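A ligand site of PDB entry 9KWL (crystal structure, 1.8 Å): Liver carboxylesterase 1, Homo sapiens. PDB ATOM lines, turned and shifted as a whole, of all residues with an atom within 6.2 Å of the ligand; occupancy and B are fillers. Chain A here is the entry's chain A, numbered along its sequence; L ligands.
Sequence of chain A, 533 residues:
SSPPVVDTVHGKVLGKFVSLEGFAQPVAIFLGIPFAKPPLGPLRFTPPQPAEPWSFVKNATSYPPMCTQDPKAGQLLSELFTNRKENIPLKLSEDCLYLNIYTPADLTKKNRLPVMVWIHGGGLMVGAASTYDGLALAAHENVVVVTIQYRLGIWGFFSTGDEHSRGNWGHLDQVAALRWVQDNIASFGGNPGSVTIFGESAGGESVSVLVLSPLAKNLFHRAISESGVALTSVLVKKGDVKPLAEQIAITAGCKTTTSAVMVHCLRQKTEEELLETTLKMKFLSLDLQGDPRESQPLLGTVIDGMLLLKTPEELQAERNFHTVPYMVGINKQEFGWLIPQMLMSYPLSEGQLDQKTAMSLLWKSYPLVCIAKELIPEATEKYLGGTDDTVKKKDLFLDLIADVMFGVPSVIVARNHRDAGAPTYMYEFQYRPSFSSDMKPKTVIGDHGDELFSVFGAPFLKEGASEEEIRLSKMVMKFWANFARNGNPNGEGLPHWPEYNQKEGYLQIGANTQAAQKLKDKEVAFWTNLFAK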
ATOM      1  N   LEU A  77     -13.714 -37.530  25.342  1.00  0.00           N
ATOM      2  CA  LEU A  77     -14.154 -36.741  24.196  1.00  0.00           C
ATOM      3  C   LEU A  77     -13.678 -37.360  22.886  1.00  0.00           C
ATOM      4  O   LEU A  77     -14.438 -37.399  21.899  1.00  0.00           O
ATOM      5  CB  LEU A  77     -13.683 -35.289  24.299  1.00  0.00           C
ATOM      6  CG  LEU A  77     -14.336 -34.414  23.228  1.00  0.00           C
ATOM      7  CD1 LEU A  77     -15.856 -34.315  23.453  1.00  0.00           C
ATOM      8  CD2 LEU A  77     -13.710 -33.029  23.236  1.00  0.00           C
ATOM      9  N   PHE A  81     -16.269 -38.495  19.880  1.00  0.00           N
ATOM     10  CA  PHE A  81     -16.270 -37.713  18.641  1.00  0.00           C
ATOM     11  C   PHE A  81     -15.544 -38.395  17.475  1.00  0.00           C
ATOM     12  O   PHE A  81     -15.688 -37.918  16.345  1.00  0.00           O
ATOM     13  CB  PHE A  81     -15.607 -36.340  18.868  1.00  0.00           C
ATOM     14  CG  PHE A  81     -16.524 -35.292  19.471  1.00  0.00           C
ATOM     15  CD1 PHE A  81     -17.863 -35.577  19.730  1.00  0.00           C
ATOM     16  CD2 PHE A  81     -16.043 -34.032  19.749  1.00  0.00           C
ATOM     17  CE1 PHE A  81     -18.702 -34.593  20.276  1.00  0.00           C
ATOM     18  CE2 PHE A  81     -16.880 -33.042  20.288  1.00  0.00           C
ATOM     19  CZ  PHE A  81     -18.199 -33.327  20.550  1.00  0.00           C
ATOM     20  N   HIS A 120     -10.206 -28.664  15.981  1.00  0.00           N
ATOM     21  CA  HIS A 120     -10.967 -29.448  16.909  1.00  0.00           C
ATOM     22  C   HIS A 120     -11.579 -28.701  18.065  1.00  0.00           C
ATOM     23  O   HIS A 120     -11.094 -27.647  18.434  1.00  0.00           O
ATOM     24  CB  HIS A 120     -10.140 -30.610  17.478  1.00  0.00           C
ATOM     25  CG  HIS A 120      -9.090 -30.196  18.453  1.00  0.00           C
ATOM     26  ND1 HIS A 120      -9.343 -29.924  19.731  1.00  0.00           N
ATOM     27  CD2 HIS A 120      -7.708 -30.075  18.296  1.00  0.00           C
ATOM     28  CE1 HIS A 120      -8.210 -29.606  20.358  1.00  0.00           C
ATOM     29  NE2 HIS A 120      -7.216 -29.716  19.474  1.00  0.00           N
ATOM     30  N   GLY A 121     -12.670 -29.248  18.600  1.00  0.00           N
ATOM     31  CA  GLY A 121     -13.328 -28.734  19.771  1.00  0.00           C
ATOM     32  C   GLY A 121     -12.793 -29.282  21.112  1.00  0.00           C
ATOM     33  O   GLY A 121     -11.840 -30.045  21.094  1.00  0.00           O
ATOM     34  N   GLY A 122     -13.486 -29.066  22.218  1.00  0.00           N
ATOM     35  CA  GLY A 122     -12.953 -29.397  23.524  1.00  0.00           C
ATOM     36  C   GLY A 122     -12.920 -28.318  24.599  1.00  0.00           C
ATOM     37  O   GLY A 122     -12.164 -28.425  25.533  1.00  0.00           O
ATOM     38  N   GLY A 123     -13.552 -27.202  24.337  1.00  0.00           N
ATOM     39  CA  GLY A 123     -13.692 -26.179  25.345  1.00  0.00           C
ATOM     40  C   GLY A 123     -12.446 -25.358  25.480  1.00  0.00           C
ATOM     41  O   GLY A 123     -12.340 -24.633  26.443  1.00  0.00           O
ATOM     42  N   LEU A 124     -11.485 -25.587  24.606  1.00  0.00           N
ATOM     43  CA  LEU A 124     -10.187 -24.915  24.646  1.00  0.00           C
ATOM     44  C   LEU A 124      -9.345 -25.583  25.757  1.00  0.00           C
ATOM     45  O   LEU A 124      -8.258 -25.140  26.034  1.00  0.00           O
ATOM     46  CB  LEU A 124     -10.286 -23.412  24.777  1.00  0.00           C
ATOM     47  CG  LEU A 124     -11.004 -22.665  23.656  1.00  0.00           C
ATOM     48  CD1 LEU A 124     -11.086 -21.179  23.938  1.00  0.00           C
ATOM     49  CD2 LEU A 124     -10.375 -22.938  22.303  1.00  0.00           C
ATOM     50  N   VAL A 126      -9.412 -29.441  26.161  1.00  0.00           N
ATOM     51  CA  VAL A 126      -9.151 -30.809  25.782  1.00  0.00           C
ATOM     52  C   VAL A 126      -9.327 -30.989  24.276  1.00  0.00           C
ATOM     53  O   VAL A 126      -9.758 -30.100  23.608  1.00  0.00           O
ATOM     54  CB  VAL A 126     -10.073 -31.829  26.483  1.00  0.00           C
ATOM     55  CG1 VAL A 126      -9.859 -31.874  27.986  1.00  0.00           C
ATOM     56  CG2 VAL A 126     -11.532 -31.595  26.124  1.00  0.00           C
ATOM     57  N   GLU A 200     -15.657 -27.329  15.169  1.00  0.00           N
ATOM     58  CA  GLU A 200     -16.879 -27.586  15.921  1.00  0.00           C
ATOM     59  C   GLU A 200     -16.642 -27.209  17.377  1.00  0.00           C
ATOM     60  O   GLU A 200     -15.541 -27.391  17.897  1.00  0.00           O
ATOM     61  CB  GLU A 200     -17.258 -29.050  15.812  1.00  0.00           C
ATOM     62  CG  GLU A 200     -18.608 -29.367  16.403  1.00  0.00           C
ATOM     63  CD  GLU A 200     -18.495 -29.947  17.788  1.00  0.00           C
ATOM     64  OE1 GLU A 200     -17.343 -30.218  18.231  1.00  0.00           O
ATOM     65  OE2 GLU A 200     -19.554 -30.193  18.402  1.00  0.00           O
ATOM     66  N   SER A 201     -17.674 -26.660  18.020  1.00  0.00           N
ATOM     67  CA  SER A 201     -17.656 -26.313  19.456  1.00  0.00           C
ATOM     68  C   SER A 201     -16.587 -25.252  19.642  1.00  0.00           C
ATOM     69  O   SER A 201     -16.648 -24.217  18.951  1.00  0.00           O
ATOM     70  CB  SER A 201     -17.499 -27.592  20.288  1.00  0.00           C
ATOM     71  OG  SER A 201     -17.789 -27.393  21.669  1.00  0.00           O
ATOM     72  N   ALA A 202     -15.590 -25.439  20.512  1.00  0.00           N
ATOM     73  CA  ALA A 202     -14.543 -24.438  20.641  1.00  0.00           C
ATOM     74  C   ALA A 202     -13.792 -24.241  19.328  1.00  0.00           C
ATOM     75  O   ALA A 202     -13.289 -23.147  19.052  1.00  0.00           O
ATOM     76  CB  ALA A 202     -13.578 -24.813  21.766  1.00  0.00           C
ATOM     77  N   GLY A 203     -13.767 -25.283  18.473  1.00  0.00           N
ATOM     78  CA  GLY A 203     -13.159 -25.115  17.165  1.00  0.00           C
ATOM     79  C   GLY A 203     -13.961 -24.185  16.280  1.00  0.00           C
ATOM     80  O   GLY A 203     -13.399 -23.389  15.524  1.00  0.00           O
ATOM     81  N   SER A 227     -21.671 -25.256  15.516  1.00  0.00           N
ATOM     82  CA  SER A 227     -22.038 -25.250  16.922  1.00  0.00           C
ATOM     83  C   SER A 227     -21.066 -24.483  17.847  1.00  0.00           C
ATOM     84  O   SER A 227     -20.683 -24.983  18.865  1.00  0.00           O
ATOM     85  CB  SER A 227     -22.269 -26.691  17.369  1.00  0.00           C
ATOM     86  OG  SER A 227     -23.147 -27.366  16.499  1.00  0.00           O
ATOM     87  N   THR A 232     -20.378 -17.090  21.708  1.00  0.00           N
ATOM     88  CA  THR A 232     -20.700 -18.127  22.655  1.00  0.00           C
ATOM     89  C   THR A 232     -19.870 -17.620  23.820  1.00  0.00           C
ATOM     90  O   THR A 232     -18.684 -17.832  23.915  1.00  0.00           O
ATOM     91  CB  THR A 232     -20.310 -19.527  22.090  1.00  0.00           C
ATOM     92  OG1 THR A 232     -21.135 -19.847  20.972  1.00  0.00           O
ATOM     93  CG2 THR A 232     -20.438 -20.601  23.154  1.00  0.00           C
ATOM     94  N   VAL A 234     -19.300 -18.248  27.101  1.00  0.00           N
ATOM     95  CA  VAL A 234     -18.472 -19.013  28.032  1.00  0.00           C
ATOM     96  C   VAL A 234     -17.039 -19.161  27.512  1.00  0.00           C
ATOM     97  O   VAL A 234     -16.122 -19.364  28.307  1.00  0.00           O
ATOM     98  CB  VAL A 234     -19.111 -20.382  28.303  1.00  0.00           C
ATOM     99  CG1 VAL A 234     -19.053 -21.260  27.051  1.00  0.00           C
ATOM    100  CG2 VAL A 234     -18.421 -21.074  29.482  1.00  0.00           C
ATOM    101  N   LEU A 235     -16.826 -19.005  26.205  1.00  0.00           N
ATOM    102  CA  LEU A 235     -15.496 -19.173  25.630  1.00  0.00           C
ATOM    103  C   LEU A 235     -14.739 -17.855  25.503  1.00  0.00           C
ATOM    104  O   LEU A 235     -13.545 -17.886  25.172  1.00  0.00           O
ATOM    105  CB  LEU A 235     -15.599 -19.850  24.258  1.00  0.00           C
ATOM    106  CG  LEU A 235     -16.008 -21.332  24.279  1.00  0.00           C
ATOM    107  CD1 LEU A 235     -16.377 -21.845  22.880  1.00  0.00           C
ATOM    108  CD2 LEU A 235     -14.921 -22.209  24.892  1.00  0.00           C
ATOM    109  N   LEU A 284     -14.280 -27.412  33.214  1.00  0.00           N
ATOM    110  CA  LEU A 284     -15.260 -28.142  32.411  1.00  0.00           C
ATOM    111  C   LEU A 284     -16.320 -28.836  33.255  1.00  0.00           C
ATOM    112  O   LEU A 284     -17.146 -29.563  32.700  1.00  0.00           O
ATOM    113  CB  LEU A 284     -14.592 -29.196  31.517  1.00  0.00           C
ATOM    114  CG  LEU A 284     -13.830 -28.696  30.294  1.00  0.00           C
ATOM    115  CD1 LEU A 284     -13.576 -29.855  29.321  1.00  0.00           C
ATOM    116  CD2 LEU A 284     -14.571 -27.534  29.629  1.00  0.00           C
ATOM    117  N   PRO A 297     -15.252 -22.116  34.376  1.00  0.00           N
ATOM    118  CA  PRO A 297     -15.230 -23.496  33.839  1.00  0.00           C
ATOM    119  C   PRO A 297     -14.111 -23.766  32.851  1.00  0.00           C
ATOM    120  O   PRO A 297     -13.826 -24.939  32.598  1.00  0.00           O
ATOM    121  CB  PRO A 297     -16.607 -23.630  33.176  1.00  0.00           C
ATOM    122  CG  PRO A 297     -17.012 -22.255  32.849  1.00  0.00           C
ATOM    123  CD  PRO A 297     -16.424 -21.360  33.911  1.00  0.00           C
ATOM    124  N   LEU A 298     -13.482 -22.738  32.279  1.00  0.00           N
ATOM    125  CA  LEU A 298     -12.381 -22.976  31.348  1.00  0.00           C
ATOM    126  C   LEU A 298     -11.572 -21.705  31.208  1.00  0.00           C
ATOM    127  O   LEU A 298     -12.053 -20.599  31.480  1.00  0.00           O
ATOM    128  CB  LEU A 298     -12.907 -23.432  29.987  1.00  0.00           C
ATOM    129  CG  LEU A 298     -14.031 -22.561  29.413  1.00  0.00           C
ATOM    130  CD1 LEU A 298     -13.449 -21.431  28.561  1.00  0.00           C
ATOM    131  CD2 LEU A 298     -15.026 -23.402  28.629  1.00  0.00           C
ATOM    132  N   LEU A 338     -24.664 -34.620  25.696  1.00  0.00           N
ATOM    133  CA  LEU A 338     -23.229 -34.701  25.899  1.00  0.00           C
ATOM    134  C   LEU A 338     -22.565 -33.623  26.683  1.00  0.00           C
ATOM    135  O   LEU A 338     -21.794 -33.926  27.569  1.00  0.00           O
ATOM    136  CB  LEU A 338     -22.571 -34.752  24.509  1.00  0.00           C
ATOM    137  CG  LEU A 338     -21.062 -34.887  24.355  1.00  0.00           C
ATOM    138  CD1 LEU A 338     -20.753 -35.859  23.239  1.00  0.00           C
ATOM    139  CD2 LEU A 338     -20.424 -33.540  24.081  1.00  0.00           C
ATOM    140  N   ILE A 339     -22.861 -32.370  26.424  1.00  0.00           N
ATOM    141  CA  ILE A 339     -22.219 -31.400  27.277  1.00  0.00           C
ATOM    142  C   ILE A 339     -22.669 -31.428  28.756  1.00  0.00           C
ATOM    143  O   ILE A 339     -21.845 -31.590  29.638  1.00  0.00           O
ATOM    144  CB  ILE A 339     -22.416 -29.969  26.716  1.00  0.00           C
ATOM    145  CG1 ILE A 339     -21.825 -29.852  25.320  1.00  0.00           C
ATOM    146  CG2 ILE A 339     -21.782 -28.931  27.627  1.00  0.00           C
ATOM    147  CD1 ILE A 339     -22.141 -28.526  24.667  1.00  0.00           C
ATOM    148  N   LEU A 343     -19.484 -34.120  29.569  1.00  0.00           N
ATOM    149  CA  LEU A 343     -18.516 -33.106  29.953  1.00  0.00           C
ATOM    150  C   LEU A 343     -18.606 -32.337  31.271  1.00  0.00           C
ATOM    151  O   LEU A 343     -17.636 -32.204  31.952  1.00  0.00           O
ATOM    152  CB  LEU A 343     -18.451 -32.074  28.837  1.00  0.00           C
ATOM    153  CG  LEU A 343     -18.114 -32.593  27.451  1.00  0.00           C
ATOM    154  CD1 LEU A 343     -18.097 -31.443  26.459  1.00  0.00           C
ATOM    155  CD2 LEU A 343     -16.777 -33.313  27.439  1.00  0.00           C
ATOM    156  N   MET A 344     -19.805 -31.886  31.609  1.00  0.00           N
ATOM    157  CA  MET A 344     -19.925 -30.970  32.742  1.00  0.00           C
ATOM    158  C   MET A 344     -20.545 -31.434  34.038  1.00  0.00           C
ATOM    159  O   MET A 344     -20.665 -30.651  34.957  1.00  0.00           O
ATOM    160  CB  MET A 344     -20.673 -29.739  32.259  1.00  0.00           C
ATOM    161  CG  MET A 344     -19.997 -28.967  31.161  1.00  0.00           C
ATOM    162  SD  MET A 344     -20.837 -27.407  30.843  1.00  0.00           S
ATOM    163  CE  MET A 344     -19.545 -26.544  29.958  1.00  0.00           C
ATOM    164  N   LEU A 368     -22.081 -20.174  32.115  1.00  0.00           N
ATOM    165  CA  LEU A 368     -22.475 -20.562  30.761  1.00  0.00           C
ATOM    166  C   LEU A 368     -23.421 -19.564  30.095  1.00  0.00           C
ATOM    167  O   LEU A 368     -23.313 -19.336  28.883  1.00  0.00           O
ATOM    168  CB  LEU A 368     -23.156 -21.924  30.784  1.00  0.00           C
ATOM    169  CG  LEU A 368     -22.359 -23.161  31.210  1.00  0.00           C
ATOM    170  CD1 LEU A 368     -23.166 -24.420  30.940  1.00  0.00           C
ATOM    171  CD2 LEU A 368     -21.051 -23.224  30.458  1.00  0.00           C
ATOM    172  N   MET A 405     -26.421 -20.415  24.639  1.00  0.00           N
ATOM    173  CA  MET A 405     -25.010 -20.669  24.325  1.00  0.00           C
ATOM    174  C   MET A 405     -24.731 -20.752  22.826  1.00  0.00           C
ATOM    175  O   MET A 405     -23.673 -20.298  22.369  1.00  0.00           O
ATOM    176  CB  MET A 405     -24.524 -21.950  24.989  1.00  0.00           C
ATOM    177  CG  MET A 405     -24.791 -22.052  26.459  1.00  0.00           C
ATOM    178  SD  MET A 405     -24.014 -23.574  27.052  1.00  0.00           S
ATOM    179  CE  MET A 405     -22.349 -23.423  26.372  1.00  0.00           C
ATOM    180  N   PHE A 406     -25.631 -21.345  22.045  1.00  0.00           N
ATOM    181  CA  PHE A 406     -25.351 -21.669  20.650  1.00  0.00           C
ATOM    182  C   PHE A 406     -26.304 -21.024  19.665  1.00  0.00           C
ATOM    183  O   PHE A 406     -25.836 -20.366  18.724  1.00  0.00           O
ATOM    184  CB  PHE A 406     -25.356 -23.197  20.472  1.00  0.00           C
ATOM    185  CG  PHE A 406     -24.281 -23.885  21.251  1.00  0.00           C
ATOM    186  CD1 PHE A 406     -22.941 -23.746  20.903  1.00  0.00           C
ATOM    187  CD2 PHE A 406     -24.589 -24.620  22.398  1.00  0.00           C
ATOM    188  CE1 PHE A 406     -21.939 -24.360  21.635  1.00  0.00           C
ATOM    189  CE2 PHE A 406     -23.609 -25.231  23.141  1.00  0.00           C
ATOM    190  CZ  PHE A 406     -22.266 -25.112  22.768  1.00  0.00           C
ATOM    191  N   HIS A 448     -25.169 -31.991  20.535  1.00  0.00           N
ATOM    192  CA  HIS A 448     -23.869 -31.398  20.226  1.00  0.00           C
ATOM    193  C   HIS A 448     -22.929 -32.452  19.672  1.00  0.00           C
ATOM    194  O   HIS A 448     -22.753 -33.523  20.271  1.00  0.00           O
ATOM    195  CB  HIS A 448     -23.285 -30.775  21.492  1.00  0.00           C
ATOM    196  CG  HIS A 448     -22.162 -29.808  21.254  1.00  0.00           C
ATOM    197  ND1 HIS A 448     -22.344 -28.622  20.573  1.00  0.00           N
ATOM    198  CD2 HIS A 448     -20.880 -29.816  21.667  1.00  0.00           C
ATOM    199  CE1 HIS A 448     -21.198 -27.948  20.554  1.00  0.00           C
ATOM    200  NE2 HIS A 448     -20.298 -28.657  21.216  1.00  0.00           N
HETATM  201  C1  LIG L   1     -17.953 -25.840  23.803  1.00  0.00           C
HETATM  202  C2  LIG L   1     -18.400 -25.183  24.935  1.00  0.00           C
HETATM  203  C3  LIG L   1     -18.317 -25.780  26.181  1.00  0.00           C
HETATM  204  C4  LIG L   1     -17.787 -27.053  26.304  1.00  0.00           C
HETATM  205  C5  LIG L   1     -17.340 -27.710  25.171  1.00  0.00           C
HETATM  206  C6  LIG L   1     -17.421 -27.116  23.912  1.00  0.00           C
HETATM  207  C7  LIG L   1     -16.947 -27.838  22.665  1.00  0.00           C
HETATM  208  C8  LIG L   1     -17.017 -29.340  22.850  1.00  0.00           C
HETATM  209  F1  LIG L   1     -16.178 -29.778  23.801  1.00  0.00           F
HETATM  210  F2  LIG L   1     -18.244 -29.717  23.224  1.00  0.00           F
HETATM  211  F3  LIG L   1     -16.724 -30.009  21.733  1.00  0.00           F
HETATM  212  O1  LIG L   1     -15.648 -27.388  22.354  1.00  0.00           O
HETATM  213 CL1  LIG L   1     -19.048 -23.605  24.758  1.00  0.00          CL
HETATM  214 CL2  LIG L   1     -18.876 -24.960  27.593  1.00  0.00          CL
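An oxygen (O1) of the ligand is in hydrogen-bond range of the backbone NH (N) of Ala 202 (2.7 Å).
The backbone NH of Gly 123 is in hydrogen-bond range of an oxygen (O1) of the ligand (2.9 Å).
The side-chain hydroxyl (OG) of Ser 201 is bonded to a carbon (C7) of the ligand.
N of Gly 122 is in hydrogen-bond range of O1 of the ligand (2.7 Å).
NE2 of His 448 is in hydrogen-bond range of OE2 of Glu 200, at 3.3 Å.
OG1 of Thr 232 is in hydrogen-bond range of O of Met 405, at 2.9 Å.
NE2 of His 448 sits at hydrogen-bond distance from OG of Ser 201 (2.8 Å).
The backbone NH (N) of Met 344 lies within hydrogen-bond range of the backbone carbonyl oxygen (O) of Ile 339, at 2.9 Å.
The backbone carbonyl oxygen (O) of Glu 200 sits close to the backbone NH (N) of Gly 121, at 3.5 Å.
The backbone NH of Leu 343 sits at hydrogen-bond distance from the backbone carbonyl oxygen of Leu 338 (3.1 Å).
A ring nitrogen (NE2) of His 448 sits close to a fluorine (F2) of the ligand, 3.1 Å away.
Phe 81 touches the ligand.
Gly 121 touches the ligand (C to O1, 3.6 Å).
OE1 of Glu 200 touches F3 of the ligand, at 3.6 Å.
Thr 232 touches the ligand (CG2 to CL1, 3.7 Å).
Val 234 touches the ligand (CG1 to CL1, 3.3 Å).
Leu 235 touches the ligand (CD1 to CL1, 3.7 Å).
Leu 343 touches the ligand (CD1 to F2, 3.7 Å).
Met 344 touches the ligand.
Leu 368 touches the ligand (CD2 to CL2, 3.99 Å).
CE of Met 405 touches CL1 of the ligand, at 3.7 Å.
15 residues have an atom within 4 Å of the ligand: Phe 81, Gly 121, Gly 122, Gly 123, Glu 200, Ser 201, Ala 202, Thr 232, Val 234, Leu 235, Leu 343, Met 344, Leu 368, Met 405 and His 448.
The nearest printed residue that does not touch the ligand is Phe 406 (4.1 Å).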
